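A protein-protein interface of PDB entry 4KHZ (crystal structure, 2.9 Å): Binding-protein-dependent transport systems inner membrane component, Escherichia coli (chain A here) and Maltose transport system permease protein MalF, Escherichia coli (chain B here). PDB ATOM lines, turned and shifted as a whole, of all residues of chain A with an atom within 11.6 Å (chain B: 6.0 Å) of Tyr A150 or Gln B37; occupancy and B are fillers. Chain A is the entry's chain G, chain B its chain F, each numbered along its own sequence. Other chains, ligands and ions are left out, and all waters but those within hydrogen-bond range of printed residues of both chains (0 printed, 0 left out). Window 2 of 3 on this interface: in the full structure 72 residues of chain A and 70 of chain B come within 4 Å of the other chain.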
ATOM      1  N   TYR A 141     -17.192 -30.272  24.256  1.00  0.00           N
ATOM      2  CA  TYR A 141     -16.260 -29.149  24.152  1.00  0.00           C
ATOM      3  C   TYR A 141     -15.451 -29.277  22.867  1.00  0.00           C
ATOM      4  O   TYR A 141     -15.339 -28.320  22.102  1.00  0.00           O
ATOM      5  CB  TYR A 141     -15.315 -29.106  25.358  1.00  0.00           C
ATOM      6  CG  TYR A 141     -14.339 -27.944  25.332  1.00  0.00           C
ATOM      7  CD1 TYR A 141     -14.719 -26.678  25.777  1.00  0.00           C
ATOM      8  CD2 TYR A 141     -13.037 -28.111  24.866  1.00  0.00           C
ATOM      9  CE1 TYR A 141     -13.832 -25.611  25.755  1.00  0.00           C
ATOM     10  CE2 TYR A 141     -12.142 -27.051  24.840  1.00  0.00           C
ATOM     11  CZ  TYR A 141     -12.543 -25.803  25.285  1.00  0.00           C
ATOM     12  OH  TYR A 141     -11.656 -24.747  25.262  1.00  0.00           O
ATOM     13  N   ALA A 142     -14.906 -30.469  22.636  1.00  0.00           N
ATOM     14  CA  ALA A 142     -14.164 -30.765  21.413  1.00  0.00           C
ATOM     15  C   ALA A 142     -15.022 -30.545  20.168  1.00  0.00           C
ATOM     16  O   ALA A 142     -14.561 -29.960  19.192  1.00  0.00           O
ATOM     17  CB  ALA A 142     -13.642 -32.193  21.447  1.00  0.00           C
ATOM     18  N   LEU A 143     -16.270 -31.009  20.210  1.00  0.00           N
ATOM     19  CA  LEU A 143     -17.193 -30.852  19.081  1.00  0.00           C
ATOM     20  C   LEU A 143     -17.418 -29.379  18.746  1.00  0.00           C
ATOM     21  O   LEU A 143     -17.222 -28.962  17.606  1.00  0.00           O
ATOM     22  CB  LEU A 143     -18.537 -31.529  19.377  1.00  0.00           C
ATOM     23  CG  LEU A 143     -19.689 -31.255  18.406  1.00  0.00           C
ATOM     24  CD1 LEU A 143     -19.315 -31.672  16.993  1.00  0.00           C
ATOM     25  CD2 LEU A 143     -20.950 -31.969  18.866  1.00  0.00           C
ATOM     26  N   PHE A 144     -17.822 -28.602  19.747  1.00  0.00           N
ATOM     27  CA  PHE A 144     -18.132 -27.184  19.550  1.00  0.00           C
ATOM     28  C   PHE A 144     -16.891 -26.300  19.390  1.00  0.00           C
ATOM     29  O   PHE A 144     -16.996 -25.175  18.899  1.00  0.00           O
ATOM     30  CB  PHE A 144     -19.023 -26.664  20.684  1.00  0.00           C
ATOM     31  CG  PHE A 144     -20.463 -27.070  20.548  1.00  0.00           C
ATOM     32  CD1 PHE A 144     -20.956 -28.182  21.213  1.00  0.00           C
ATOM     33  CD2 PHE A 144     -21.322 -26.344  19.738  1.00  0.00           C
ATOM     34  CE1 PHE A 144     -22.283 -28.556  21.079  1.00  0.00           C
ATOM     35  CE2 PHE A 144     -22.649 -26.714  19.598  1.00  0.00           C
ATOM     36  CZ  PHE A 144     -23.131 -27.823  20.270  1.00  0.00           C
ATOM     37  N   ASP A 145     -15.727 -26.797  19.803  1.00  0.00           N
ATOM     38  CA  ASP A 145     -14.471 -26.077  19.590  1.00  0.00           C
ATOM     39  C   ASP A 145     -14.097 -26.122  18.110  1.00  0.00           C
ATOM     40  O   ASP A 145     -13.792 -25.089  17.512  1.00  0.00           O
ATOM     41  CB  ASP A 145     -13.346 -26.674  20.444  1.00  0.00           C
ATOM     42  CG  ASP A 145     -12.049 -25.875  20.366  1.00  0.00           C
ATOM     43  OD1 ASP A 145     -12.101 -24.648  20.133  1.00  0.00           O
ATOM     44  OD2 ASP A 145     -10.972 -26.478  20.555  1.00  0.00           O
ATOM     45  N   ARG A 146     -14.132 -27.319  17.525  1.00  0.00           N
ATOM     46  CA  ARG A 146     -13.827 -27.496  16.101  1.00  0.00           C
ATOM     47  C   ARG A 146     -14.966 -27.003  15.206  1.00  0.00           C
ATOM     48  O   ARG A 146     -14.721 -26.499  14.111  1.00  0.00           O
ATOM     49  CB  ARG A 146     -13.498 -28.963  15.780  1.00  0.00           C
ATOM     50  CG  ARG A 146     -12.083 -29.395  16.156  1.00  0.00           C
ATOM     51  CD  ARG A 146     -11.996 -29.919  17.582  1.00  0.00           C
ATOM     52  NE  ARG A 146     -10.634 -30.321  17.945  1.00  0.00           N
ATOM     53  CZ  ARG A 146      -9.933 -29.860  18.985  1.00  0.00           C
ATOM     54  NH1 ARG A 146     -10.441 -28.965  19.831  1.00  0.00           N
ATOM     55  NH2 ARG A 146      -8.700 -30.312  19.193  1.00  0.00           N
ATOM     56  N   LEU A 147     -16.205 -27.148  15.671  1.00  0.00           N
ATOM     57  CA  LEU A 147     -17.376 -26.674  14.928  1.00  0.00           C
ATOM     58  C   LEU A 147     -17.502 -25.148  14.968  1.00  0.00           C
ATOM     59  O   LEU A 147     -18.147 -24.553  14.104  1.00  0.00           O
ATOM     60  CB  LEU A 147     -18.649 -27.331  15.479  1.00  0.00           C
ATOM     61  CG  LEU A 147     -19.995 -27.009  14.817  1.00  0.00           C
ATOM     62  CD1 LEU A 147     -20.847 -28.265  14.684  1.00  0.00           C
ATOM     63  CD2 LEU A 147     -20.758 -25.933  15.580  1.00  0.00           C
ATOM     64  N   GLY A 148     -16.878 -24.522  15.964  1.00  0.00           N
ATOM     65  CA  GLY A 148     -16.977 -23.079  16.163  1.00  0.00           C
ATOM     66  C   GLY A 148     -16.259 -22.240  15.122  1.00  0.00           C
ATOM     67  O   GLY A 148     -16.797 -21.241  14.652  1.00  0.00           O
ATOM     68  N   GLU A 149     -15.040 -22.636  14.765  1.00  0.00           N
ATOM     69  CA  GLU A 149     -14.225 -21.858  13.822  1.00  0.00           C
ATOM     70  C   GLU A 149     -14.793 -21.834  12.400  1.00  0.00           C
ATOM     71  O   GLU A 149     -14.578 -20.873  11.661  1.00  0.00           O
ATOM     72  CB  GLU A 149     -12.767 -22.340  13.818  1.00  0.00           C
ATOM     73  CG  GLU A 149     -12.551 -23.789  13.409  1.00  0.00           C
ATOM     74  CD  GLU A 149     -11.114 -24.234  13.615  1.00  0.00           C
ATOM     75  OE1 GLU A 149     -10.205 -23.605  13.030  1.00  0.00           O
ATOM     76  OE2 GLU A 149     -10.893 -25.213  14.361  1.00  0.00           O
ATOM     77  N   TYR A 150     -15.518 -22.884  12.021  1.00  0.00           N
ATOM     78  CA  TYR A 150     -16.192 -22.926  10.724  1.00  0.00           C
ATOM     79  C   TYR A 150     -17.514 -22.164  10.760  1.00  0.00           C
ATOM     80  O   TYR A 150     -17.829 -21.423   9.829  1.00  0.00           O
ATOM     81  CB  TYR A 150     -16.431 -24.370  10.284  1.00  0.00           C
ATOM     82  CG  TYR A 150     -15.153 -25.134  10.037  1.00  0.00           C
ATOM     83  CD1 TYR A 150     -14.761 -26.167  10.880  1.00  0.00           C
ATOM     84  CD2 TYR A 150     -14.326 -24.814   8.965  1.00  0.00           C
ATOM     85  CE1 TYR A 150     -13.586 -26.866  10.659  1.00  0.00           C
ATOM     86  CE2 TYR A 150     -13.149 -25.506   8.735  1.00  0.00           C
ATOM     87  CZ  TYR A 150     -12.784 -26.531   9.585  1.00  0.00           C
ATOM     88  OH  TYR A 150     -11.615 -27.222   9.360  1.00  0.00           O
ATOM     89  N   ILE A 151     -18.277 -22.349  11.836  1.00  0.00           N
ATOM     90  CA  ILE A 151     -19.575 -21.689  12.006  1.00  0.00           C
ATOM     91  C   ILE A 151     -19.596 -20.932  13.345  1.00  0.00           C
ATOM     92  O   ILE A 151     -20.046 -21.472  14.359  1.00  0.00           O
ATOM     93  CB  ILE A 151     -20.737 -22.708  11.938  1.00  0.00           C
ATOM     94  CG1 ILE A 151     -20.513 -23.707  10.794  1.00  0.00           C
ATOM     95  CG2 ILE A 151     -22.067 -21.990  11.750  1.00  0.00           C
ATOM     96  CD1 ILE A 151     -21.588 -24.768  10.680  1.00  0.00           C
ATOM     97  N   PRO A 152     -19.093 -19.679  13.352  1.00  0.00           N
ATOM     98  CA  PRO A 152     -18.936 -18.869  14.569  1.00  0.00           C
ATOM     99  C   PRO A 152     -20.178 -18.725  15.453  1.00  0.00           C
ATOM    100  O   PRO A 152     -20.051 -18.730  16.678  1.00  0.00           O
ATOM    101  CB  PRO A 152     -18.532 -17.495  14.024  1.00  0.00           C
ATOM    102  CG  PRO A 152     -17.835 -17.796  12.747  1.00  0.00           C
ATOM    103  CD  PRO A 152     -18.539 -18.990  12.169  1.00  0.00           C
ATOM    104  N   PHE A 153     -21.358 -18.606  14.848  1.00  0.00           N
ATOM    105  CA  PHE A 153     -22.572 -18.275  15.609  1.00  0.00           C
ATOM    106  C   PHE A 153     -23.174 -19.443  16.408  1.00  0.00           C
ATOM    107  O   PHE A 153     -24.137 -19.247  17.152  1.00  0.00           O
ATOM    108  CB  PHE A 153     -23.630 -17.599  14.709  1.00  0.00           C
ATOM    109  CG  PHE A 153     -24.308 -18.523  13.729  1.00  0.00           C
ATOM    110  CD1 PHE A 153     -23.757 -18.763  12.475  1.00  0.00           C
ATOM    111  CD2 PHE A 153     -25.526 -19.118  14.044  1.00  0.00           C
ATOM    112  CE1 PHE A 153     -24.389 -19.600  11.569  1.00  0.00           C
ATOM    113  CE2 PHE A 153     -26.162 -19.958  13.142  1.00  0.00           C
ATOM    114  CZ  PHE A 153     -25.593 -20.198  11.902  1.00  0.00           C
ATOM    115  N   ILE A 154     -22.607 -20.642  16.266  1.00  0.00           N
ATOM    116  CA  ILE A 154     -23.046 -21.810  17.041  1.00  0.00           C
ATOM    117  C   ILE A 154     -21.859 -22.593  17.609  1.00  0.00           C
ATOM    118  O   ILE A 154     -21.873 -23.824  17.628  1.00  0.00           O
ATOM    119  CB  ILE A 154     -23.928 -22.761  16.197  1.00  0.00           C
ATOM    120  CG1 ILE A 154     -23.232 -23.121  14.880  1.00  0.00           C
ATOM    121  CG2 ILE A 154     -25.284 -22.129  15.925  1.00  0.00           C
ATOM    122  CD1 ILE A 154     -23.810 -24.342  14.199  1.00  0.00           C
ATOM    123  N   GLY A 155     -20.841 -21.875  18.077  1.00  0.00           N
ATOM    124  CA  GLY A 155     -19.630 -22.500  18.610  1.00  0.00           C
ATOM    125  C   GLY A 155     -19.565 -22.421  20.122  1.00  0.00           C
ATOM    126  O   GLY A 155     -20.598 -22.319  20.790  1.00  0.00           O
ATOM    127  N   LEU A 156     -18.349 -22.479  20.662  1.00  0.00           N
ATOM    128  CA  LEU A 156     -18.131 -22.284  22.095  1.00  0.00           C
ATOM    129  C   LEU A 156     -18.388 -20.830  22.462  1.00  0.00           C
ATOM    130  O   LEU A 156     -18.155 -19.931  21.654  1.00  0.00           O
ATOM    131  CB  LEU A 156     -16.700 -22.661  22.497  1.00  0.00           C
ATOM    132  CG  LEU A 156     -16.352 -24.147  22.562  1.00  0.00           C
ATOM    133  CD1 LEU A 156     -14.864 -24.315  22.824  1.00  0.00           C
ATOM    134  CD2 LEU A 156     -17.171 -24.858  23.629  1.00  0.00           C
ATOM    135  N   THR A 158     -21.194 -19.269  22.821  1.00  0.00           N
ATOM    136  CA  THR A 158     -22.315 -18.687  22.081  1.00  0.00           C
ATOM    137  C   THR A 158     -23.618 -19.359  22.490  1.00  0.00           C
ATOM    138  O   THR A 158     -23.630 -20.535  22.861  1.00  0.00           O
ATOM    139  CB  THR A 158     -22.159 -18.847  20.556  1.00  0.00           C
ATOM    140  OG1 THR A 158     -22.167 -20.239  20.207  1.00  0.00           O
ATOM    141  CG2 THR A 158     -20.870 -18.205  20.070  1.00  0.00           C
ATOM    142  N   LEU B  30     -17.287 -26.109   2.657  1.00  0.00           N
ATOM    143  CA  LEU B  30     -16.956 -26.407   4.051  1.00  0.00           C
ATOM    144  C   LEU B  30     -16.420 -27.829   4.216  1.00  0.00           C
ATOM    145  O   LEU B  30     -15.672 -28.102   5.152  1.00  0.00           O
ATOM    146  CB  LEU B  30     -18.182 -26.214   4.952  1.00  0.00           C
ATOM    147  CG  LEU B  30     -18.680 -24.778   5.150  1.00  0.00           C
ATOM    148  CD1 LEU B  30     -20.057 -24.772   5.797  1.00  0.00           C
ATOM    149  CD2 LEU B  30     -17.697 -23.965   5.980  1.00  0.00           C
ATOM    150  N   LEU B  33     -12.597 -28.094   3.368  1.00  0.00           N
ATOM    151  CA  LEU B  33     -11.837 -27.474   4.461  1.00  0.00           C
ATOM    152  C   LEU B  33     -11.648 -28.408   5.664  1.00  0.00           C
ATOM    153  O   LEU B  33     -10.807 -28.143   6.522  1.00  0.00           O
ATOM    154  CB  LEU B  33     -12.504 -26.170   4.916  1.00  0.00           C
ATOM    155  CG  LEU B  33     -12.371 -24.982   3.958  1.00  0.00           C
ATOM    156  CD1 LEU B  33     -13.370 -23.891   4.314  1.00  0.00           C
ATOM    157  CD2 LEU B  33     -10.952 -24.433   3.960  1.00  0.00           C
ATOM    158  N   MET B  34     -12.435 -29.483   5.730  1.00  0.00           N
ATOM    159  CA  MET B  34     -12.250 -30.518   6.751  1.00  0.00           C
ATOM    160  C   MET B  34     -11.045 -31.387   6.397  1.00  0.00           C
ATOM    161  O   MET B  34     -10.264 -31.752   7.273  1.00  0.00           O
ATOM    162  CB  MET B  34     -13.491 -31.412   6.889  1.00  0.00           C
ATOM    163  CG  MET B  34     -14.829 -30.688   6.974  1.00  0.00           C
ATOM    164  SD  MET B  34     -14.894 -29.349   8.180  1.00  0.00           S
ATOM    165  CE  MET B  34     -14.880 -30.265   9.716  1.00  0.00           C
ATOM    166  N   TYR B  35     -10.913 -31.724   5.113  1.00  0.00           N
ATOM    167  CA  TYR B  35      -9.769 -32.496   4.608  1.00  0.00           C
ATOM    168  C   TYR B  35      -8.472 -31.720   4.815  1.00  0.00           C
ATOM    169  O   TYR B  35      -7.474 -32.276   5.278  1.00  0.00           O
ATOM    170  CB  TYR B  35      -9.956 -32.826   3.122  1.00  0.00           C
ATOM    171  CG  TYR B  35      -8.916 -33.766   2.544  1.00  0.00           C
ATOM    172  CD1 TYR B  35      -9.047 -35.147   2.671  1.00  0.00           C
ATOM    173  CD2 TYR B  35      -7.808 -33.273   1.855  1.00  0.00           C
ATOM    174  CE1 TYR B  35      -8.102 -36.010   2.139  1.00  0.00           C
ATOM    175  CE2 TYR B  35      -6.857 -34.130   1.319  1.00  0.00           C
ATOM    176  CZ  TYR B  35      -7.009 -35.495   1.463  1.00  0.00           C
ATOM    177  OH  TYR B  35      -6.069 -36.348   0.934  1.00  0.00           O
ATOM    178  N   ALA B  36      -8.497 -30.434   4.467  1.00  0.00           N
ATOM    179  CA  ALA B  36      -7.394 -29.527   4.776  1.00  0.00           C
ATOM    180  C   ALA B  36      -7.379 -29.242   6.275  1.00  0.00           C
ATOM    181  O   ALA B  36      -8.396 -29.404   6.952  1.00  0.00           O
ATOM    182  CB  ALA B  36      -7.531 -28.232   3.990  1.00  0.00           C
ATOM    183  N   GLN B  37      -6.222 -28.829   6.784  1.00  0.00           N
ATOM    184  CA  GLN B  37      -6.040 -28.544   8.213  1.00  0.00           C
ATOM    185  C   GLN B  37      -6.246 -29.795   9.081  1.00  0.00           C
ATOM    186  O   GLN B  37      -6.701 -29.699  10.223  1.00  0.00           O
ATOM    187  CB  GLN B  37      -6.982 -27.417   8.667  1.00  0.00           C
ATOM    188  CG  GLN B  37      -6.964 -26.181   7.776  1.00  0.00           C
ATOM    189  CD  GLN B  37      -8.223 -25.340   7.899  1.00  0.00           C
ATOM    190  OE1 GLN B  37      -9.335 -25.867   7.944  1.00  0.00           O
ATOM    191  NE2 GLN B  37      -8.053 -24.024   7.940  1.00  0.00           N
ATOM    192  N   GLY B  38      -5.902 -30.961   8.533  1.00  0.00           N
ATOM    193  CA  GLY B  38      -6.024 -32.233   9.249  1.00  0.00           C
ATOM    194  C   GLY B  38      -7.467 -32.656   9.464  1.00  0.00           C
ATOM    195  O   GLY B  38      -8.166 -32.990   8.509  1.00  0.00           O
ATOM    196  N   GLU B  39      -7.891 -32.657  10.728  1.00  0.00           N
ATOM    197  CA  GLU B  39      -9.281 -32.920  11.134  1.00  0.00           C
ATOM    198  C   GLU B  39     -10.022 -33.988  10.321  1.00  0.00           C
ATOM    199  O   GLU B  39     -11.118 -33.744   9.808  1.00  0.00           O
ATOM    200  CB  GLU B  39     -10.079 -31.610  11.148  1.00  0.00           C
ATOM    201  CG  GLU B  39      -9.588 -30.610  12.182  1.00  0.00           C
ATOM    202  CD  GLU B  39     -10.512 -29.418  12.337  1.00  0.00           C
ATOM    203  OE1 GLU B  39     -11.157 -29.022  11.343  1.00  0.00           O
ATOM    204  OE2 GLU B  39     -10.590 -28.871  13.458  1.00  0.00           O
ATOM    205  N   PHE B  42     -13.550 -35.187  12.083  1.00  0.00           N
ATOM    206  CA  PHE B  42     -14.810 -34.474  11.859  1.00  0.00           C
ATOM    207  C   PHE B  42     -15.019 -34.162  10.368  1.00  0.00           C
ATOM    208  O   PHE B  42     -15.796 -33.276  10.014  1.00  0.00           O
ATOM    209  CB  PHE B  42     -14.810 -33.187  12.702  1.00  0.00           C
ATOM    210  CG  PHE B  42     -16.179 -32.597  12.938  1.00  0.00           C
ATOM    211  CD1 PHE B  42     -17.194 -33.354  13.513  1.00  0.00           C
ATOM    212  CD2 PHE B  42     -16.442 -31.271  12.612  1.00  0.00           C
ATOM    213  CE1 PHE B  42     -18.448 -32.808  13.733  1.00  0.00           C
ATOM    214  CE2 PHE B  42     -17.694 -30.720  12.833  1.00  0.00           C
ATOM    215  CZ  PHE B  42     -18.698 -31.489  13.395  1.00  0.00           C
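Among the printed residues, merely in contact across the chains: Leu A143 with Phe B42, Arg A146 with Glu B39, Glu A149 with Glu B39 and Tyr A150 with Met B34.
Of the 17 printed residues of chain A, 4 touch a printed residue of chain B.
Hydrophobic or aromatic side chains of chain A within 4 Å of the printed part of chain B: Leu A143 and Tyr A150.
Printed residues of chain B that touch a printed residue of chain A: Leu B33, Met B34, Gln B37, Glu B39 and Phe B42.
Among the printed residues, 7 pairs touch across the chains.
OD2 of Asp A145 lies within salt-bridge range of NH1 of Arg A146 (2.6 Å).
OE1 of Gln B37 sits close to O of Leu B33 (3.1 Å).
The side-chain amide oxygen of Gln B37 lies within hydrogen-bond range of the side-chain hydroxyl of Tyr A150, at 3.0 Å.
The side-chain hydroxyl (OH) of Tyr A150 is in hydrogen-bond range of the side-chain carboxylate (OE1) of Glu B39.
O of Leu B33 is in hydrogen-bond range of OH of Tyr A150, at 3.1 Å.
Of the printed residues of chain B, Leu A143 touches Phe B42 (3.6 Å).
Printed residues of chain B within 4 Å of Arg A146: Glu B39.
Of the printed residues of chain B, Glu A149 touches Glu B39.
Tyr A150 touches just these residues of chain B: Leu B33, Met B34, Gln B37 and Glu B39.
No residue of chain A comes within 4 Å of Leu B30.
Leu B33 touches just one residue of chain A: Tyr A150 (3.1 Å).
Printed residues of chain A within 4 Å of Gln B37: Tyr A150.
Gly B38 touches none of the printed residues of chain A.
Of chain A, only Arg A146 (3.1 Å), Glu A149 (3.8 Å) and Tyr A150 (2.7 Å) come within 4 Å of Glu B39.
Printed residues of chain A within 4 Å of Phe B42: Leu A143 (3.6 Å).
The nearest residue of chain A that does not touch Gln B37 is Glu A149 (5.5 Å).
The nearest printed residue of chain A that does not touch Phe B42 is Leu A147 (4.1 Å).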
